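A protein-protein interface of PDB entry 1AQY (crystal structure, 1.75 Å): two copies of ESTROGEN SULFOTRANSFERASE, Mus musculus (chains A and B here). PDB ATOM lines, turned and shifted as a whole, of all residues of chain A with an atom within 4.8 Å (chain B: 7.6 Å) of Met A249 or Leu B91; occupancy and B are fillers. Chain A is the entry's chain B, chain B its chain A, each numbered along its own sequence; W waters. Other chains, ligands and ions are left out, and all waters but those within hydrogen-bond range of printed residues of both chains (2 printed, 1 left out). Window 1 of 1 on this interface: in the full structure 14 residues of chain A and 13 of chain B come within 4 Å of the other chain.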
ATOM      1  N   PHE A  78     -14.885  16.686   1.721  1.00  0.00           N
ATOM      2  CA  PHE A  78     -14.561  16.892   0.314  1.00  0.00           C
ATOM      3  C   PHE A  78     -13.116  17.360   0.088  1.00  0.00           C
ATOM      4  O   PHE A  78     -12.672  17.501  -1.052  1.00  0.00           O
ATOM      5  CB  PHE A  78     -15.563  17.852  -0.371  1.00  0.00           C
ATOM      6  CG  PHE A  78     -15.744  19.192   0.323  1.00  0.00           C
ATOM      7  CD1 PHE A  78     -14.792  20.207   0.188  1.00  0.00           C
ATOM      8  CD2 PHE A  78     -16.900  19.457   1.068  1.00  0.00           C
ATOM      9  CE1 PHE A  78     -14.989  21.471   0.780  1.00  0.00           C
ATOM     10  CE2 PHE A  78     -17.108  20.715   1.664  1.00  0.00           C
ATOM     11  CZ  PHE A  78     -16.148  21.722   1.517  1.00  0.00           C
ATOM     12  N   ILE A  92     -12.787  25.453  -8.432  1.00  0.00           N
ATOM     13  CA  ILE A  92     -12.844  24.070  -7.933  1.00  0.00           C
ATOM     14  C   ILE A  92     -12.172  23.123  -8.932  1.00  0.00           C
ATOM     15  O   ILE A  92     -12.471  23.167 -10.126  1.00  0.00           O
ATOM     16  CB  ILE A  92     -14.307  23.597  -7.729  1.00  0.00           C
ATOM     17  CG1 ILE A  92     -15.040  24.545  -6.779  1.00  0.00           C
ATOM     18  CG2 ILE A  92     -14.331  22.155  -7.172  1.00  0.00           C
ATOM     19  CD1 ILE A  92     -16.523  24.236  -6.662  1.00  0.00           C
ATOM     20  N   MET A 147     -31.890  21.171  -4.205  1.00  0.00           N
ATOM     21  CA  MET A 147     -30.831  21.743  -3.358  1.00  0.00           C
ATOM     22  C   MET A 147     -29.721  22.473  -4.128  1.00  0.00           C
ATOM     23  O   MET A 147     -29.218  23.505  -3.669  1.00  0.00           O
ATOM     24  CB  MET A 147     -30.199  20.637  -2.498  1.00  0.00           C
ATOM     25  CG  MET A 147     -29.170  21.126  -1.487  1.00  0.00           C
ATOM     26  SD  MET A 147     -28.123  19.808  -0.811  1.00  0.00           S
ATOM     27  CE  MET A 147     -29.359  18.626  -0.315  1.00  0.00           C
ATOM     28  N   ILE A 148     -29.320  21.938  -5.280  1.00  0.00           N
ATOM     29  CA  ILE A 148     -28.276  22.574  -6.086  1.00  0.00           C
ATOM     30  C   ILE A 148     -28.839  23.788  -6.841  1.00  0.00           C
ATOM     31  O   ILE A 148     -29.680  23.654  -7.737  1.00  0.00           O
ATOM     32  CB  ILE A 148     -27.661  21.564  -7.084  1.00  0.00           C
ATOM     33  CG1 ILE A 148     -27.128  20.344  -6.318  1.00  0.00           C
ATOM     34  CG2 ILE A 148     -26.537  22.232  -7.889  1.00  0.00           C
ATOM     35  CD1 ILE A 148     -26.077  20.658  -5.258  1.00  0.00           C
ATOM     36  N   THR A 149     -28.358  24.979  -6.482  1.00  0.00           N
ATOM     37  CA  THR A 149     -28.854  26.220  -7.082  1.00  0.00           C
ATOM     38  C   THR A 149     -28.748  26.335  -8.608  1.00  0.00           C
ATOM     39  O   THR A 149     -29.666  26.864  -9.252  1.00  0.00           O
ATOM     40  CB  THR A 149     -28.183  27.467  -6.422  1.00  0.00           C
ATOM     41  OG1 THR A 149     -26.771  27.431  -6.649  1.00  0.00           O
ATOM     42  CG2 THR A 149     -28.443  27.484  -4.912  1.00  0.00           C
ATOM     43  N   MET A 244     -20.095  23.250   5.416  1.00  0.00           N
ATOM     44  CA  MET A 244     -18.802  23.906   5.138  1.00  0.00           C
ATOM     45  C   MET A 244     -18.741  24.282   3.650  1.00  0.00           C
ATOM     46  O   MET A 244     -17.702  24.719   3.139  1.00  0.00           O
ATOM     47  CB  MET A 244     -17.623  22.975   5.466  1.00  0.00           C
ATOM     48  CG  MET A 244     -17.436  22.667   6.948  1.00  0.00           C
ATOM     49  SD  MET A 244     -16.759  24.040   7.931  1.00  0.00           S
ATOM     50  CE  MET A 244     -18.242  24.828   8.512  1.00  0.00           C
ATOM     51  N   MET A 245     -19.869  24.087   2.965  1.00  0.00           N
ATOM     52  CA  MET A 245     -20.004  24.404   1.544  1.00  0.00           C
ATOM     53  C   MET A 245     -21.043  25.529   1.400  1.00  0.00           C
ATOM     54  O   MET A 245     -22.176  25.390   1.856  1.00  0.00           O
ATOM     55  CB  MET A 245     -20.453  23.156   0.774  1.00  0.00           C
ATOM     56  CG  MET A 245     -20.712  23.395  -0.699  1.00  0.00           C
ATOM     57  SD  MET A 245     -19.182  23.497  -1.660  1.00  0.00           S
ATOM     58  CE  MET A 245     -18.388  21.959  -1.212  1.00  0.00           C
ATOM     59  N   PRO A 246     -20.655  26.667   0.780  1.00  0.00           N
ATOM     60  CA  PRO A 246     -21.501  27.853   0.550  1.00  0.00           C
ATOM     61  C   PRO A 246     -22.949  27.620   0.138  1.00  0.00           C
ATOM     62  O   PRO A 246     -23.238  26.783  -0.713  1.00  0.00           O
ATOM     63  CB  PRO A 246     -20.738  28.637  -0.515  1.00  0.00           C
ATOM     64  CG  PRO A 246     -19.315  28.301  -0.247  1.00  0.00           C
ATOM     65  CD  PRO A 246     -19.288  26.875   0.264  1.00  0.00           C
ATOM     66  N   GLU A 247     -23.844  28.394   0.744  1.00  0.00           N
ATOM     67  CA  GLU A 247     -25.272  28.323   0.465  1.00  0.00           C
ATOM     68  C   GLU A 247     -25.590  28.852  -0.928  1.00  0.00           C
ATOM     69  O   GLU A 247     -26.675  28.602  -1.462  1.00  0.00           O
ATOM     70  CB  GLU A 247     -26.049  29.131   1.501  1.00  0.00           C
ATOM     71  CG  GLU A 247     -27.130  28.342   2.218  1.00  0.00           C
ATOM     72  CD  GLU A 247     -28.271  29.219   2.719  1.00  0.00           C
ATOM     73  OE1 GLU A 247     -28.436  30.350   2.202  1.00  0.00           O
ATOM     74  OE2 GLU A 247     -29.006  28.769   3.631  1.00  0.00           O
ATOM     75  N   GLU A 248     -24.652  29.597  -1.510  1.00  0.00           N
ATOM     76  CA  GLU A 248     -24.835  30.142  -2.857  1.00  0.00           C
ATOM     77  C   GLU A 248     -24.829  28.989  -3.869  1.00  0.00           C
ATOM     78  O   GLU A 248     -25.388  29.094  -4.958  1.00  0.00           O
ATOM     79  CB  GLU A 248     -23.703  31.123  -3.204  1.00  0.00           C
ATOM     80  CG  GLU A 248     -23.717  32.428  -2.419  1.00  0.00           C
ATOM     81  CD  GLU A 248     -22.529  32.543  -1.485  1.00  0.00           C
ATOM     82  OE1 GLU A 248     -22.479  31.772  -0.496  1.00  0.00           O
ATOM     83  OE2 GLU A 248     -21.649  33.396  -1.741  1.00  0.00           O
ATOM     84  N   MET A 249     -24.186  27.892  -3.488  1.00  0.00           N
ATOM     85  CA  MET A 249     -24.092  26.711  -4.339  1.00  0.00           C
ATOM     86  C   MET A 249     -25.058  25.600  -3.923  1.00  0.00           C
ATOM     87  O   MET A 249     -25.756  25.022  -4.758  1.00  0.00           O
ATOM     88  CB  MET A 249     -22.672  26.147  -4.299  1.00  0.00           C
ATOM     89  CG  MET A 249     -21.612  27.129  -3.856  1.00  0.00           C
ATOM     90  SD  MET A 249     -20.233  27.103  -4.988  1.00  0.00           S
ATOM     91  CE  MET A 249     -20.994  27.784  -6.426  1.00  0.00           C
ATOM     92  N   MET A 250     -25.074  25.318  -2.623  1.00  0.00           N
ATOM     93  CA  MET A 250     -25.893  24.264  -2.023  1.00  0.00           C
ATOM     94  C   MET A 250     -26.788  24.867  -0.943  1.00  0.00           C
ATOM     95  O   MET A 250     -26.330  25.113   0.168  1.00  0.00           O
ATOM     96  CB  MET A 250     -24.952  23.226  -1.404  1.00  0.00           C
ATOM     97  CG  MET A 250     -25.548  21.863  -1.126  1.00  0.00           C
ATOM     98  SD  MET A 250     -24.258  20.636  -0.749  1.00  0.00           S
ATOM     99  CE  MET A 250     -22.977  21.092  -1.916  1.00  0.00           C
ATOM    100  N   ASN A 251     -28.058  25.092  -1.264  1.00  0.00           N
ATOM    101  CA  ASN A 251     -29.006  25.690  -0.313  1.00  0.00           C
ATOM    102  C   ASN A 251     -29.793  24.686   0.550  1.00  0.00           C
ATOM    103  O   ASN A 251     -30.863  24.210   0.148  1.00  0.00           O
ATOM    104  CB  ASN A 251     -29.989  26.576  -1.074  1.00  0.00           C
ATOM    105  CG  ASN A 251     -30.823  27.434  -0.158  1.00  0.00           C
ATOM    106  OD1 ASN A 251     -30.822  27.249   1.060  1.00  0.00           O
ATOM    107  ND2 ASN A 251     -31.543  28.385  -0.737  1.00  0.00           N
ATOM    108  N   ARG B  87     -12.384  34.511   2.991  1.00  0.00           N
ATOM    109  CA  ARG B  87     -12.715  33.211   3.572  1.00  0.00           C
ATOM    110  C   ARG B  87     -14.209  32.911   3.473  1.00  0.00           C
ATOM    111  O   ARG B  87     -15.044  33.781   3.723  1.00  0.00           O
ATOM    112  CB  ARG B  87     -12.280  33.185   5.049  1.00  0.00           C
ATOM    113  CG  ARG B  87     -12.720  31.948   5.858  1.00  0.00           C
ATOM    114  CD  ARG B  87     -11.737  30.789   5.675  1.00  0.00           C
ATOM    115  NE  ARG B  87     -12.019  29.651   6.551  1.00  0.00           N
ATOM    116  CZ  ARG B  87     -11.347  29.386   7.668  1.00  0.00           C
ATOM    117  NH1 ARG B  87     -10.352  30.175   8.058  1.00  0.00           N
ATOM    118  NH2 ARG B  87     -11.663  28.315   8.395  1.00  0.00           N
ATOM    119  N   ASN B  88     -14.539  31.684   3.070  1.00  0.00           N
ATOM    120  CA  ASN B  88     -15.928  31.229   2.992  1.00  0.00           C
ATOM    121  C   ASN B  88     -15.905  29.764   3.424  1.00  0.00           C
ATOM    122  O   ASN B  88     -15.880  28.866   2.586  1.00  0.00           O
ATOM    123  CB  ASN B  88     -16.482  31.354   1.571  1.00  0.00           C
ATOM    124  CG  ASN B  88     -18.004  31.408   1.551  1.00  0.00           C
ATOM    125  OD1 ASN B  88     -18.664  30.878   2.451  1.00  0.00           O
ATOM    126  ND2 ASN B  88     -18.568  32.051   0.532  1.00  0.00           N
ATOM    127  N   GLU B  89     -15.893  29.554   4.744  1.00  0.00           N
ATOM    128  CA  GLU B  89     -15.824  28.229   5.366  1.00  0.00           C
ATOM    129  C   GLU B  89     -14.676  27.408   4.759  1.00  0.00           C
ATOM    130  O   GLU B  89     -13.531  27.888   4.717  1.00  0.00           O
ATOM    131  CB  GLU B  89     -17.167  27.494   5.257  1.00  0.00           C
ATOM    132  CG  GLU B  89     -18.288  28.076   6.154  1.00  0.00           C
ATOM    133  CD  GLU B  89     -17.928  28.148   7.642  1.00  0.00           C
ATOM    134  OE1 GLU B  89     -16.984  27.452   8.088  1.00  0.00           O
ATOM    135  OE2 GLU B  89     -18.599  28.907   8.380  1.00  0.00           O
ATOM    136  N   ASP B  90     -14.958  26.192   4.279  1.00  0.00           N
ATOM    137  CA  ASP B  90     -13.898  25.346   3.711  1.00  0.00           C
ATOM    138  C   ASP B  90     -13.765  25.352   2.192  1.00  0.00           C
ATOM    139  O   ASP B  90     -12.929  24.635   1.656  1.00  0.00           O
ATOM    140  CB  ASP B  90     -14.055  23.899   4.192  1.00  0.00           C
ATOM    141  CG  ASP B  90     -13.583  23.708   5.626  1.00  0.00           C
ATOM    142  OD1 ASP B  90     -12.956  24.634   6.181  1.00  0.00           O
ATOM    143  OD2 ASP B  90     -13.838  22.631   6.206  1.00  0.00           O
ATOM    144  N   LEU B  91     -14.582  26.148   1.501  1.00  0.00           N
ATOM    145  CA  LEU B  91     -14.510  26.236   0.042  1.00  0.00           C
ATOM    146  C   LEU B  91     -13.471  27.270  -0.432  1.00  0.00           C
ATOM    147  O   LEU B  91     -12.798  27.061  -1.436  1.00  0.00           O
ATOM    148  CB  LEU B  91     -15.882  26.584  -0.545  1.00  0.00           C
ATOM    149  CG  LEU B  91     -15.903  26.665  -2.079  1.00  0.00           C
ATOM    150  CD1 LEU B  91     -15.636  25.295  -2.664  1.00  0.00           C
ATOM    151  CD2 LEU B  91     -17.239  27.185  -2.565  1.00  0.00           C
ATOM    152  N   ILE B  92     -13.351  28.386   0.284  1.00  0.00           N
ATOM    153  CA  ILE B  92     -12.385  29.439  -0.059  1.00  0.00           C
ATOM    154  C   ILE B  92     -11.577  29.830   1.187  1.00  0.00           C
ATOM    155  O   ILE B  92     -12.147  30.078   2.247  1.00  0.00           O
ATOM    156  CB  ILE B  92     -13.093  30.706  -0.590  1.00  0.00           C
ATOM    157  CG1 ILE B  92     -13.934  30.365  -1.821  1.00  0.00           C
ATOM    158  CG2 ILE B  92     -12.067  31.779  -0.945  1.00  0.00           C
ATOM    159  CD1 ILE B  92     -14.791  31.530  -2.300  1.00  0.00           C
ATOM    160  N   ASN B  93     -10.256  29.891   1.050  1.00  0.00           N
ATOM    161  CA  ASN B  93      -9.383  30.231   2.172  1.00  0.00           C
ATOM    162  C   ASN B  93      -8.037  30.810   1.688  1.00  0.00           C
ATOM    163  O   ASN B  93      -7.137  30.074   1.280  1.00  0.00           O
ATOM    164  CB  ASN B  93      -9.155  28.973   3.023  1.00  0.00           C
ATOM    165  CG  ASN B  93      -8.514  29.268   4.376  1.00  0.00           C
ATOM    166  OD1 ASN B  93      -8.750  28.548   5.351  1.00  0.00           O
ATOM    167  ND2 ASN B  93      -7.686  30.310   4.440  1.00  0.00           N
ATOM    168  N   GLN B  97      -3.980  29.184   1.124  1.00  0.00           N
ATOM    169  CA  GLN B  97      -3.311  29.328  -0.168  1.00  0.00           C
ATOM    170  C   GLN B  97      -1.914  29.909   0.006  1.00  0.00           C
ATOM    171  O   GLN B  97      -0.982  29.504  -0.680  1.00  0.00           O
ATOM    172  CB  GLN B  97      -4.092  30.268  -1.072  1.00  0.00           C
ATOM    173  CG  GLN B  97      -5.297  29.677  -1.757  1.00  0.00           C
ATOM    174  CD  GLN B  97      -5.949  30.680  -2.692  1.00  0.00           C
ATOM    175  OE1 GLN B  97      -5.659  30.710  -3.889  1.00  0.00           O
ATOM    176  NE2 GLN B  97      -6.826  31.514  -2.147  1.00  0.00           N
ATOM    177  N   PRO B 246     -17.347  31.581 -10.580  1.00  0.00           N
ATOM    178  CA  PRO B 246     -18.768  31.214 -10.704  1.00  0.00           C
ATOM    179  C   PRO B 246     -19.796  32.342 -10.658  1.00  0.00           C
ATOM    180  O   PRO B 246     -19.721  33.242  -9.815  1.00  0.00           O
ATOM    181  CB  PRO B 246     -18.985  30.221  -9.568  1.00  0.00           C
ATOM    182  CG  PRO B 246     -17.667  29.572  -9.413  1.00  0.00           C
ATOM    183  CD  PRO B 246     -16.620  30.615  -9.734  1.00  0.00           C
ATOM    184  N   GLU B 247     -20.770  32.258 -11.563  1.00  0.00           N
ATOM    185  CA  GLU B 247     -21.842  33.239 -11.660  1.00  0.00           C
ATOM    186  C   GLU B 247     -22.781  33.152 -10.459  1.00  0.00           C
ATOM    187  O   GLU B 247     -23.554  34.079 -10.195  1.00  0.00           O
ATOM    188  CB  GLU B 247     -22.638  33.019 -12.949  1.00  0.00           C
ATOM    189  CG  GLU B 247     -22.734  34.249 -13.833  1.00  0.00           C
ATOM    190  CD  GLU B 247     -23.985  34.258 -14.696  1.00  0.00           C
ATOM    191  OE1 GLU B 247     -24.950  33.533 -14.363  1.00  0.00           O
ATOM    192  OE2 GLU B 247     -24.001  34.991 -15.708  1.00  0.00           O
ATOM    193  N   GLU B 248     -22.718  32.032  -9.741  1.00  0.00           N
ATOM    194  CA  GLU B 248     -23.558  31.842  -8.559  1.00  0.00           C
ATOM    195  C   GLU B 248     -23.114  32.809  -7.461  1.00  0.00           C
ATOM    196  O   GLU B 248     -23.891  33.159  -6.567  1.00  0.00           O
ATOM    197  CB  GLU B 248     -23.443  30.405  -8.035  1.00  0.00           C
ATOM    198  CG  GLU B 248     -24.049  29.340  -8.938  1.00  0.00           C
ATOM    199  CD  GLU B 248     -22.988  28.424  -9.531  1.00  0.00           C
ATOM    200  OE1 GLU B 248     -22.208  28.892 -10.389  1.00  0.00           O
ATOM    201  OE2 GLU B 248     -22.935  27.237  -9.134  1.00  0.00           O
ATOM    202  N   MET B 249     -21.855  33.229  -7.540  1.00  0.00           N
ATOM    203  CA  MET B 249     -21.269  34.148  -6.570  1.00  0.00           C
ATOM    204  C   MET B 249     -21.157  35.571  -7.104  1.00  0.00           C
ATOM    205  O   MET B 249     -21.526  36.530  -6.426  1.00  0.00           O
ATOM    206  CB  MET B 249     -19.871  33.676  -6.177  1.00  0.00           C
ATOM    207  CG  MET B 249     -19.589  32.210  -6.438  1.00  0.00           C
ATOM    208  SD  MET B 249     -18.825  31.467  -5.001  1.00  0.00           S
ATOM    209  CE  MET B 249     -20.206  31.544  -3.879  1.00  0.00           C
HETATM  210  O   HOH W   1     -22.164  36.183  -3.405  1.00  0.00           O
HETATM  211  O   HOH W   2     -24.806  25.438  -7.552  1.00  0.00           O
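The side-chain hydroxyl (OG1) of Thr A149 is in hydrogen-bond range of the backbone carbonyl oxygen (O) of Glu A248 (2.7 Å).
The guanidinium group (NE) of Arg B87 lies within hydrogen-bond range of the backbone carbonyl oxygen (O) of Glu B89 (3.0 Å).
The backbone NH of Thr A149 sits at hydrogen-bond distance from the backbone carbonyl oxygen of Met A249 (3.1 Å).
SD of Met A244 lies close to OE1 of Glu B89 (3.4 Å).
O of Met A244 sits at hydrogen-bond distance from N of Asp B90 (3.3 Å).
Water W2 lies within hydrogen-bond range of the side-chain hydroxyl (OG1) of Thr A149 (2.9 Å), the backbone carbonyl oxygen (O) of Met A249 (3.0 Å) and the side-chain carboxylate (OE2) of Glu B248 (3.0 Å).
Water W1 lies within hydrogen-bond range of O of Met B249 and OE2 of Glu A248.
Met A249 touches just these residues of chain B: Leu B91 and Glu B248.
Leu B91 touches three residues of chain A.
Printed residues of chain A within 4 Å of Glu B89: Met A244.
Of the printed residues of chain B, Pro A246 touches Asn B88 and Leu B91.
Printed residues of chain B within 4 Å of Glu A248: Glu B248 and Met B249.
Of the printed residues of chain A, Met B249 touches Glu A248.
Printed residues of chain A within 4 Å of Asp B90: Phe A78 and Met A244.
The nearest residue of chain A that does not touch Leu B91 is Met A245 (4.1 Å).
Hydrophobic or aromatic side chains of chain A that line the printed part of chain B: Phe A78, Met A244, Pro A246 and Met A249.
Of the 12 printed residues of chain B, 6 touch a printed residue of chain A.
Hydrophobic or aromatic side chains of chain B that line the printed part of chain A: Leu B91 and Met B249.
Phe A78 touches Asp B90.
Leu B91 touches Met A244 (N to O, 3.8 Å).
Pro A246 touches Asn B88.
CG of Pro A246 touches CD2 of Leu B91, at 3.3 Å.
Glu B248 touches Glu A248.
Met B249 touches Glu A248.
Met A249 touches Leu B91 (SD to CD2, 3.9 Å).
Glu B248 touches Met A249 (OE2 to CE, 3.4 Å).
Glu A248 touches its own counterpart, Glu B248.
Glu A248 touches Met B249, and with the chains exchanged Met A249 touches Glu B248.
5 positions are printed for both chains.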
